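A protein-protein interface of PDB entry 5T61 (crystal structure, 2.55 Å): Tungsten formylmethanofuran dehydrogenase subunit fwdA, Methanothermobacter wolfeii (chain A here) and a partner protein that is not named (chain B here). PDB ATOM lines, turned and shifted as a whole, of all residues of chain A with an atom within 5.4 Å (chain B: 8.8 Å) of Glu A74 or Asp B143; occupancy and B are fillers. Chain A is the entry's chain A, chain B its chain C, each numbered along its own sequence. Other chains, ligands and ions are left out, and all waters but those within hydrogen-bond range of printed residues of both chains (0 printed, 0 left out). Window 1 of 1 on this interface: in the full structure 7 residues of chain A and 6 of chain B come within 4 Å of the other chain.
Among the printed residues, pairs that only touch across the chains: Pro A73 with Arg B141, Glu A74 with Arg B141, Lys A77 with Tyr B140, Glu A74 with Trp B144, Glu A74 with Asp B143, Pro A73 with Tyr B140, Glu A74 with Tyr B140 and Arg A72 with Trp B144.
Glu A74 touches just these residues of chain B: Tyr B140, Arg B141, Gly B142, Asp B143 and Trp B144.
Of the printed residues of chain A, Asp B143 touches Glu A74.
Of the printed residues of chain A, Gly B142 touches Glu A74 and Lys A334.
Of the printed residues of chain B, Lys A334 touches Gly B142 (2.8 Å).
Of the printed residues of chain A, Tyr B140 touches Pro A73 (3.8 Å), Glu A74 (3.95 Å) and Lys A77 (3.6 Å).
Ser B139 touches none of the printed residues of chain A.
Tyr B165 touches none of the printed residues of chain A.
The nearest residue of chain B that does not touch Glu A74 is Arg B145 (4.6 Å).
The nearest residue of chain A that does not touch Asp B143 is Lys A334 (4.8 Å).
O of Tyr A71 sits at hydrogen-bond distance from NZ of Lys A334, 2.9 Å away.
NE of Arg A72 is in salt-bridge range of OE2 of Glu A74 (3.2 Å).
NZ of Lys A334 lies within salt-bridge range of OE2 of Glu A74, 2.8 Å away.
The side-chain hydroxyl (OG) of Ser B139 is in hydrogen-bond range of the backbone carbonyl oxygen (O) of Asp B143 (3.4 Å).
The side-chain carboxylate (OD1) of Asp B143 is in salt-bridge range of the guanidinium group (NE) of Arg B145, 2.9 Å away.
Of the 19 printed residues of chain B, 5 touch a printed residue of chain A.
Printed residues of chain B that touch a printed residue of chain A: Tyr B140, Arg B141, Gly B142, Asp B143 and Trp B144.
Along chain B the printed residues that touch a printed residue of chain A span positions 140 to 144.
Printed residues of chain A that touch a printed residue of chain B: Arg A72, Pro A73, Glu A74, Lys A77 and Lys A334.
Among the printed residues, 10 pairs touch across the chains.
Among the printed residues, no Asp or Glu carboxylate lies within 4 Å of a Lys or Arg side-chain nitrogen of the other chain.
NZ of Lys A334 lies within hydrogen-bond range of O of Gly B142 (2.8 Å).
The backbone carbonyl oxygen of Gly B142 lies close to the side-chain carboxylate of Glu A74, 3.4 Å away.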
ATOM      1  N   TYR A  71      -7.756 -12.637  25.431  1.00  0.00           N
ATOM      2  CA  TYR A  71      -8.053 -11.612  24.438  1.00  0.00           C
ATOM      3  C   TYR A  71      -7.408 -11.892  23.082  1.00  0.00           C
ATOM      4  O   TYR A  71      -7.423 -11.018  22.209  1.00  0.00           O
ATOM      5  CB  TYR A  71      -7.687 -10.215  24.986  1.00  0.00           C
ATOM      6  CG  TYR A  71      -6.334  -9.596  24.657  1.00  0.00           C
ATOM      7  CD1 TYR A  71      -5.177 -10.355  24.565  1.00  0.00           C
ATOM      8  CD2 TYR A  71      -6.223  -8.218  24.481  1.00  0.00           C
ATOM      9  CE1 TYR A  71      -3.954  -9.767  24.275  1.00  0.00           C
ATOM     10  CE2 TYR A  71      -5.005  -7.622  24.193  1.00  0.00           C
ATOM     11  CZ  TYR A  71      -3.873  -8.404  24.091  1.00  0.00           C
ATOM     12  OH  TYR A  71      -2.654  -7.828  23.807  1.00  0.00           O
ATOM     13  N   ARG A  72      -6.857 -13.091  22.883  1.00  0.00           N
ATOM     14  CA  ARG A  72      -6.327 -13.524  21.589  1.00  0.00           C
ATOM     15  C   ARG A  72      -6.909 -14.874  21.193  1.00  0.00           C
ATOM     16  O   ARG A  72      -6.193 -15.882  21.137  1.00  0.00           O
ATOM     17  CB  ARG A  72      -4.801 -13.578  21.630  1.00  0.00           C
ATOM     18  CG  ARG A  72      -4.197 -12.259  22.025  1.00  0.00           C
ATOM     19  CD  ARG A  72      -2.843 -12.091  21.418  1.00  0.00           C
ATOM     20  NE  ARG A  72      -2.938 -12.180  19.970  1.00  0.00           N
ATOM     21  CZ  ARG A  72      -1.889 -12.303  19.170  1.00  0.00           C
ATOM     22  NH1 ARG A  72      -0.670 -12.344  19.685  1.00  0.00           N
ATOM     23  NH2 ARG A  72      -2.062 -12.390  17.859  1.00  0.00           N
ATOM     24  N   PRO A  73      -8.211 -14.928  20.883  1.00  0.00           N
ATOM     25  CA  PRO A  73      -8.776 -16.181  20.360  1.00  0.00           C
ATOM     26  C   PRO A  73      -8.237 -16.554  18.994  1.00  0.00           C
ATOM     27  O   PRO A  73      -8.152 -17.746  18.676  1.00  0.00           O
ATOM     28  CB  PRO A  73     -10.281 -15.889  20.299  1.00  0.00           C
ATOM     29  CG  PRO A  73     -10.358 -14.408  20.164  1.00  0.00           C
ATOM     30  CD  PRO A  73      -9.219 -13.857  20.960  1.00  0.00           C
ATOM     31  N   GLU A  74      -7.878 -15.564  18.169  1.00  0.00           N
ATOM     32  CA  GLU A  74      -7.310 -15.867  16.861  1.00  0.00           C
ATOM     33  C   GLU A  74      -5.962 -16.567  16.985  1.00  0.00           C
ATOM     34  O   GLU A  74      -5.604 -17.374  16.117  1.00  0.00           O
ATOM     35  CB  GLU A  74      -7.203 -14.589  16.025  1.00  0.00           C
ATOM     36  CG  GLU A  74      -6.060 -13.661  16.394  1.00  0.00           C
ATOM     37  CD  GLU A  74      -6.316 -12.866  17.662  1.00  0.00           C
ATOM     38  OE1 GLU A  74      -7.377 -13.054  18.300  1.00  0.00           O
ATOM     39  OE2 GLU A  74      -5.445 -12.051  18.023  1.00  0.00           O
ATOM     40  N   ASP A  75      -5.209 -16.286  18.052  1.00  0.00           N
ATOM     41  CA  ASP A  75      -3.962 -17.007  18.282  1.00  0.00           C
ATOM     42  C   ASP A  75      -4.232 -18.464  18.639  1.00  0.00           C
ATOM     43  O   ASP A  75      -3.424 -19.343  18.315  1.00  0.00           O
ATOM     44  CB  ASP A  75      -3.148 -16.316  19.380  1.00  0.00           C
ATOM     45  CG  ASP A  75      -1.790 -16.965  19.605  1.00  0.00           C
ATOM     46  OD1 ASP A  75      -0.968 -16.967  18.662  1.00  0.00           O
ATOM     47  OD2 ASP A  75      -1.538 -17.460  20.723  1.00  0.00           O
ATOM     48  N   SER A  76      -5.365 -18.737  19.296  1.00  0.00           N
ATOM     49  CA  SER A  76      -5.735 -20.112  19.614  1.00  0.00           C
ATOM     50  C   SER A  76      -6.214 -20.858  18.375  1.00  0.00           C
ATOM     51  O   SER A  76      -5.862 -22.025  18.171  1.00  0.00           O
ATOM     52  CB  SER A  76      -6.821 -20.124  20.687  1.00  0.00           C
ATOM     53  OG  SER A  76      -6.283 -19.841  21.963  1.00  0.00           O
ATOM     54  N   LYS A  77      -7.017 -20.198  17.537  1.00  0.00           N
ATOM     55  CA  LYS A  77      -7.489 -20.819  16.305  1.00  0.00           C
ATOM     56  C   LYS A  77      -6.326 -21.190  15.398  1.00  0.00           C
ATOM     57  O   LYS A  77      -6.407 -22.159  14.633  1.00  0.00           O
ATOM     58  CB  LYS A  77      -8.422 -19.855  15.575  1.00  0.00           C
ATOM     59  CG  LYS A  77      -9.008 -20.397  14.293  1.00  0.00           C
ATOM     60  CD  LYS A  77     -10.044 -19.441  13.734  1.00  0.00           C
ATOM     61  CE  LYS A  77     -10.244 -19.692  12.254  1.00  0.00           C
ATOM     62  NZ  LYS A  77     -11.383 -18.909  11.718  1.00  0.00           N
ATOM     63  N   ARG A  78      -5.242 -20.422  15.478  1.00  0.00           N
ATOM     64  CA  ARG A  78      -4.036 -20.695  14.709  1.00  0.00           C
ATOM     65  C   ARG A  78      -3.388 -22.012  15.109  1.00  0.00           C
ATOM     66  O   ARG A  78      -2.710 -22.643  14.289  1.00  0.00           O
ATOM     67  CB  ARG A  78      -3.060 -19.541  14.908  1.00  0.00           C
ATOM     68  CG  ARG A  78      -1.829 -19.552  14.046  1.00  0.00           C
ATOM     69  CD  ARG A  78      -0.996 -18.347  14.412  1.00  0.00           C
ATOM     70  NE  ARG A  78       0.367 -18.430  13.910  1.00  0.00           N
ATOM     71  CZ  ARG A  78       1.322 -17.567  14.236  1.00  0.00           C
ATOM     72  NH1 ARG A  78       1.053 -16.561  15.057  1.00  0.00           N
ATOM     73  NH2 ARG A  78       2.543 -17.710  13.742  1.00  0.00           N
ATOM     74  N   LYS A 334      -4.253  -4.144  19.613  1.00  0.00           N
ATOM     75  CA  LYS A 334      -5.009  -4.197  20.863  1.00  0.00           C
ATOM     76  C   LYS A 334      -4.099  -4.231  22.087  1.00  0.00           C
ATOM     77  O   LYS A 334      -3.038  -4.858  22.081  1.00  0.00           O
ATOM     78  CB  LYS A 334      -5.938  -5.410  20.857  1.00  0.00           C
ATOM     79  CG  LYS A 334      -5.241  -6.733  20.626  1.00  0.00           C
ATOM     80  CD  LYS A 334      -6.272  -7.803  20.351  1.00  0.00           C
ATOM     81  CE  LYS A 334      -5.646  -9.112  19.924  1.00  0.00           C
ATOM     82  NZ  LYS A 334      -6.715 -10.081  19.561  1.00  0.00           N
ATOM     83  N   GLN B 119     -16.799 -15.397   5.495  1.00  0.00           N
ATOM     84  CA  GLN B 119     -15.848 -14.931   6.497  1.00  0.00           C
ATOM     85  C   GLN B 119     -14.420 -15.270   6.085  1.00  0.00           C
ATOM     86  O   GLN B 119     -14.139 -16.386   5.638  1.00  0.00           O
ATOM     87  CB  GLN B 119     -16.182 -15.554   7.854  1.00  0.00           C
ATOM     88  CG  GLN B 119     -15.027 -15.594   8.843  1.00  0.00           C
ATOM     89  CD  GLN B 119     -15.373 -16.366  10.091  1.00  0.00           C
ATOM     90  OE1 GLN B 119     -15.286 -15.845  11.201  1.00  0.00           O
ATOM     91  NE2 GLN B 119     -15.787 -17.614   9.931  1.00  0.00           N
ATOM     92  N   ASP B 120     -13.520 -14.296   6.238  1.00  0.00           N
ATOM     93  CA  ASP B 120     -12.097 -14.452   5.907  1.00  0.00           C
ATOM     94  C   ASP B 120     -11.895 -14.835   4.443  1.00  0.00           C
ATOM     95  O   ASP B 120     -10.992 -15.601   4.105  1.00  0.00           O
ATOM     96  CB  ASP B 120     -11.423 -15.481   6.817  1.00  0.00           C
ATOM     97  CG  ASP B 120     -11.121 -14.939   8.194  1.00  0.00           C
ATOM     98  OD1 ASP B 120     -10.503 -13.856   8.291  1.00  0.00           O
ATOM     99  OD2 ASP B 120     -11.495 -15.608   9.178  1.00  0.00           O
ATOM    100  N   ARG B 122     -10.719 -14.763   0.650  1.00  0.00           N
ATOM    101  CA  ARG B 122      -9.476 -14.360   0.002  1.00  0.00           C
ATOM    102  C   ARG B 122      -9.597 -14.189  -1.501  1.00  0.00           C
ATOM    103  O   ARG B 122      -8.833 -13.415  -2.080  1.00  0.00           O
ATOM    104  CB  ARG B 122      -8.368 -15.387   0.270  1.00  0.00           C
ATOM    105  CG  ARG B 122      -8.337 -15.884   1.689  1.00  0.00           C
ATOM    106  CD  ARG B 122      -7.477 -15.017   2.593  1.00  0.00           C
ATOM    107  NE  ARG B 122      -7.768 -15.304   3.991  1.00  0.00           N
ATOM    108  CZ  ARG B 122      -7.453 -16.456   4.603  1.00  0.00           C
ATOM    109  NH1 ARG B 122      -6.843 -17.425   3.943  1.00  0.00           N
ATOM    110  NH2 ARG B 122      -7.768 -16.622   5.878  1.00  0.00           N
ATOM    111  N   SER B 138     -16.962 -11.218   7.165  1.00  0.00           N
ATOM    112  CA  SER B 138     -16.400 -10.684   8.394  1.00  0.00           C
ATOM    113  C   SER B 138     -15.013 -11.268   8.646  1.00  0.00           C
ATOM    114  O   SER B 138     -14.481 -12.057   7.861  1.00  0.00           O
ATOM    115  CB  SER B 138     -17.313 -10.985   9.577  1.00  0.00           C
ATOM    116  OG  SER B 138     -17.197 -12.349   9.950  1.00  0.00           O
ATOM    117  N   SER B 139     -14.412 -10.859   9.756  1.00  0.00           N
ATOM    118  CA  SER B 139     -13.202 -11.474  10.269  1.00  0.00           C
ATOM    119  C   SER B 139     -13.569 -12.504  11.336  1.00  0.00           C
ATOM    120  O   SER B 139     -14.743 -12.768  11.610  1.00  0.00           O
ATOM    121  CB  SER B 139     -12.255 -10.403  10.818  1.00  0.00           C
ATOM    122  OG  SER B 139     -12.735  -9.866  12.038  1.00  0.00           O
ATOM    123  N   TYR B 140     -12.547 -13.089  11.950  1.00  0.00           N
ATOM    124  CA  TYR B 140     -12.714 -13.980  13.088  1.00  0.00           C
ATOM    125  C   TYR B 140     -12.466 -13.217  14.386  1.00  0.00           C
ATOM    126  O   TYR B 140     -11.781 -12.190  14.395  1.00  0.00           O
ATOM    127  CB  TYR B 140     -11.771 -15.184  12.992  1.00  0.00           C
ATOM    128  CG  TYR B 140     -11.896 -16.131  14.160  1.00  0.00           C
ATOM    129  CD1 TYR B 140     -13.022 -16.928  14.312  1.00  0.00           C
ATOM    130  CD2 TYR B 140     -10.904 -16.204  15.129  1.00  0.00           C
ATOM    131  CE1 TYR B 140     -13.148 -17.784  15.387  1.00  0.00           C
ATOM    132  CE2 TYR B 140     -11.021 -17.059  16.210  1.00  0.00           C
ATOM    133  CZ  TYR B 140     -12.146 -17.846  16.332  1.00  0.00           C
ATOM    134  OH  TYR B 140     -12.273 -18.698  17.402  1.00  0.00           O
ATOM    135  N   ARG B 141     -13.070 -13.709  15.471  1.00  0.00           N
ATOM    136  CA  ARG B 141     -12.916 -13.126  16.804  1.00  0.00           C
ATOM    137  C   ARG B 141     -11.472 -12.743  17.089  1.00  0.00           C
ATOM    138  O   ARG B 141     -10.557 -13.553  16.917  1.00  0.00           O
ATOM    139  CB  ARG B 141     -13.386 -14.115  17.873  1.00  0.00           C
ATOM    140  CG  ARG B 141     -14.810 -14.554  17.730  1.00  0.00           C
ATOM    141  CD  ARG B 141     -15.701 -13.357  17.567  1.00  0.00           C
ATOM    142  NE  ARG B 141     -17.107 -13.729  17.545  1.00  0.00           N
ATOM    143  CZ  ARG B 141     -18.091 -12.869  17.312  1.00  0.00           C
ATOM    144  NH1 ARG B 141     -17.810 -11.598  17.070  1.00  0.00           N
ATOM    145  NH2 ARG B 141     -19.352 -13.280  17.317  1.00  0.00           N
ATOM    146  N   GLY B 142     -11.270 -11.496  17.509  1.00  0.00           N
ATOM    147  CA  GLY B 142      -9.969 -11.055  17.951  1.00  0.00           C
ATOM    148  C   GLY B 142      -9.026 -10.652  16.846  1.00  0.00           C
ATOM    149  O   GLY B 142      -8.077  -9.899  17.102  1.00  0.00           O
ATOM    150  N   ASP B 143      -9.229 -11.148  15.631  1.00  0.00           N
ATOM    151  CA  ASP B 143      -8.317 -10.838  14.548  1.00  0.00           C
ATOM    152  C   ASP B 143      -8.670  -9.483  13.951  1.00  0.00           C
ATOM    153  O   ASP B 143      -9.846  -9.152  13.754  1.00  0.00           O
ATOM    154  CB  ASP B 143      -8.372 -11.934  13.482  1.00  0.00           C
ATOM    155  CG  ASP B 143      -7.099 -12.020  12.657  1.00  0.00           C
ATOM    156  OD1 ASP B 143      -6.409 -10.992  12.501  1.00  0.00           O
ATOM    157  OD2 ASP B 143      -6.785 -13.129  12.170  1.00  0.00           O
ATOM    158  N   TRP B 144      -7.640  -8.691  13.674  1.00  0.00           N
ATOM    159  CA  TRP B 144      -7.804  -7.386  13.057  1.00  0.00           C
ATOM    160  C   TRP B 144      -7.595  -7.443  11.552  1.00  0.00           C
ATOM    161  O   TRP B 144      -7.735  -6.422  10.874  1.00  0.00           O
ATOM    162  CB  TRP B 144      -6.847  -6.380  13.710  1.00  0.00           C
ATOM    163  CG  TRP B 144      -5.394  -6.724  13.575  1.00  0.00           C
ATOM    164  CD1 TRP B 144      -4.518  -6.216  12.665  1.00  0.00           C
ATOM    165  CD2 TRP B 144      -4.652  -7.665  14.365  1.00  0.00           C
ATOM    166  NE1 TRP B 144      -3.274  -6.769  12.843  1.00  0.00           N
ATOM    167  CE2 TRP B 144      -3.330  -7.664  13.878  1.00  0.00           C
ATOM    168  CE3 TRP B 144      -4.974  -8.503  15.438  1.00  0.00           C
ATOM    169  CZ2 TRP B 144      -2.330  -8.465  14.427  1.00  0.00           C
ATOM    170  CZ3 TRP B 144      -3.980  -9.299  15.982  1.00  0.00           C
ATOM    171  CH2 TRP B 144      -2.674  -9.275  15.475  1.00  0.00           C
ATOM    172  N   ARG B 145      -7.286  -8.621  11.020  1.00  0.00           N
ATOM    173  CA  ARG B 145      -7.134  -8.856   9.590  1.00  0.00           C
ATOM    174  C   ARG B 145      -8.283  -9.758   9.159  1.00  0.00           C
ATOM    175  O   ARG B 145      -8.359 -10.917   9.578  1.00  0.00           O
ATOM    176  CB  ARG B 145      -5.783  -9.500   9.275  1.00  0.00           C
ATOM    177  CG  ARG B 145      -4.574  -8.731   9.786  1.00  0.00           C
ATOM    178  CD  ARG B 145      -3.441  -9.672  10.180  1.00  0.00           C
ATOM    179  NE  ARG B 145      -3.773 -10.427  11.385  1.00  0.00           N
ATOM    180  CZ  ARG B 145      -2.893 -11.100  12.119  1.00  0.00           C
ATOM    181  NH1 ARG B 145      -1.611 -11.114  11.778  1.00  0.00           N
ATOM    182  NH2 ARG B 145      -3.295 -11.756  13.200  1.00  0.00           N
ATOM    183  N   GLY B 146      -9.184  -9.223   8.344  1.00  0.00           N
ATOM    184  CA  GLY B 146     -10.326  -9.995   7.901  1.00  0.00           C
ATOM    185  C   GLY B 146     -10.277 -10.362   6.434  1.00  0.00           C
ATOM    186  O   GLY B 146      -9.215 -10.702   5.899  1.00  0.00           O
ATOM    187  N   MET B 147     -11.439 -10.308   5.786  1.00  0.00           N
ATOM    188  CA  MET B 147     -11.545 -10.559   4.356  1.00  0.00           C
ATOM    189  C   MET B 147     -10.590  -9.667   3.575  1.00  0.00           C
ATOM    190  O   MET B 147     -10.557  -8.449   3.769  1.00  0.00           O
ATOM    191  CB  MET B 147     -12.985 -10.320   3.901  1.00  0.00           C
ATOM    192  CG  MET B 147     -13.180 -10.353   2.402  1.00  0.00           C
ATOM    193  SD  MET B 147     -14.921 -10.217   1.949  1.00  0.00           S
ATOM    194  CE  MET B 147     -14.785 -10.059   0.173  1.00  0.00           C
ATOM    195  N   GLU B 164     -17.232  -6.697   8.546  1.00  0.00           N
ATOM    196  CA  GLU B 164     -16.474  -6.431   9.764  1.00  0.00           C
ATOM    197  C   GLU B 164     -14.984  -6.616   9.526  1.00  0.00           C
ATOM    198  O   GLU B 164     -14.544  -7.681   9.083  1.00  0.00           O
ATOM    199  CB  GLU B 164     -16.951  -7.357  10.887  1.00  0.00           C
ATOM    200  CG  GLU B 164     -16.284  -7.115  12.238  1.00  0.00           C
ATOM    201  CD  GLU B 164     -15.529  -8.330  12.748  1.00  0.00           C
ATOM    202  OE1 GLU B 164     -15.272  -9.253  11.944  1.00  0.00           O
ATOM    203  OE2 GLU B 164     -15.197  -8.364  13.952  1.00  0.00           O
ATOM    204  N   TYR B 165     -14.211  -5.567   9.816  1.00  0.00           N
ATOM    205  CA  TYR B 165     -12.758  -5.572   9.624  1.00  0.00           C
ATOM    206  C   TYR B 165     -12.366  -5.925   8.195  1.00  0.00           C
ATOM    207  O   TYR B 165     -11.322  -6.543   7.968  1.00  0.00           O
ATOM    208  CB  TYR B 165     -12.068  -6.524  10.602  1.00  0.00           C
ATOM    209  CG  TYR B 165     -11.853  -5.949  11.977  1.00  0.00           C
ATOM    210  CD1 TYR B 165     -10.815  -5.060  12.220  1.00  0.00           C
ATOM    211  CD2 TYR B 165     -12.678  -6.301  13.035  1.00  0.00           C
ATOM    212  CE1 TYR B 165     -10.608  -4.533  13.479  1.00  0.00           C
ATOM    213  CE2 TYR B 165     -12.481  -5.777  14.296  1.00  0.00           C
ATOM    214  CZ  TYR B 165     -11.444  -4.893  14.513  1.00  0.00           C
ATOM    215  OH  TYR B 165     -11.238  -4.370  15.768  1.00  0.00           O
ATOM    216  N   MET B 166     -13.184  -5.530   7.221  1.00  0.00           N
ATOM    217  CA  MET B 166     -12.853  -5.818   5.832  1.00  0.00           C
ATOM    218  C   MET B 166     -11.514  -5.192   5.471  1.00  0.00           C
ATOM    219  O   MET B 166     -11.175  -4.100   5.934  1.00  0.00           O
ATOM    220  CB  MET B 166     -13.935  -5.298   4.888  1.00  0.00           C
ATOM    221  CG  MET B 166     -13.744  -5.786   3.460  1.00  0.00           C
ATOM    222  SD  MET B 166     -14.883  -5.064   2.272  1.00  0.00           S
ATOM    223  CE  MET B 166     -16.332  -6.018   2.636  1.00  0.00           C
ATOM    224  N   ASN B 167     -10.758  -5.889   4.625  1.00  0.00           N
ATOM    225  CA  ASN B 167      -9.416  -5.468   4.255  1.00  0.00           C
ATOM    226  C   ASN B 167      -9.165  -5.717   2.772  1.00  0.00           C
ATOM    227  O   ASN B 167      -8.040  -6.021   2.366  1.00  0.00           O
ATOM    228  CB  ASN B 167      -8.377  -6.204   5.106  1.00  0.00           C
ATOM    229  CG  ASN B 167      -7.020  -5.536   5.084  1.00  0.00           C
ATOM    230  OD1 ASN B 167      -6.908  -4.336   4.836  1.00  0.00           O
ATOM    231  ND2 ASN B 167      -5.976  -6.317   5.337  1.00  0.00           N
ATOM    232  N   HIS B 184     -15.302  -1.263  11.689  1.00  0.00           N
ATOM    233  CA  HIS B 184     -13.847  -1.454  11.680  1.00  0.00           C
ATOM    234  C   HIS B 184     -13.280  -1.710  10.284  1.00  0.00           C
ATOM    235  O   HIS B 184     -12.235  -2.353  10.152  1.00  0.00           O
ATOM    236  CB  HIS B 184     -13.421  -2.593  12.611  1.00  0.00           C
ATOM    237  CG  HIS B 184     -13.499  -2.256  14.066  1.00  0.00           C
ATOM    238  ND1 HIS B 184     -12.645  -1.357  14.668  1.00  0.00           N
ATOM    239  CD2 HIS B 184     -14.314  -2.715  15.044  1.00  0.00           C
ATOM    240  CE1 HIS B 184     -12.936  -1.272  15.953  1.00  0.00           C
ATOM    241  NE2 HIS B 184     -13.946  -2.084  16.207  1.00  0.00           N
ATOM    242  N   ASN B 186     -11.127  -1.477   7.051  1.00  0.00           N
ATOM    243  CA  ASN B 186      -9.811  -0.958   6.695  1.00  0.00           C
ATOM    244  C   ASN B 186      -9.655  -0.706   5.207  1.00  0.00           C
ATOM    245  O   ASN B 186      -8.998   0.258   4.810  1.00  0.00           O
ATOM    246  CB  ASN B 186      -8.721  -1.938   7.141  1.00  0.00           C
ATOM    247  CG  ASN B 186      -8.294  -1.725   8.575  1.00  0.00           C
ATOM    248  OD1 ASN B 186      -8.406  -2.626   9.406  1.00  0.00           O
ATOM    249  ND2 ASN B 186      -7.800  -0.529   8.877  1.00  0.00           N
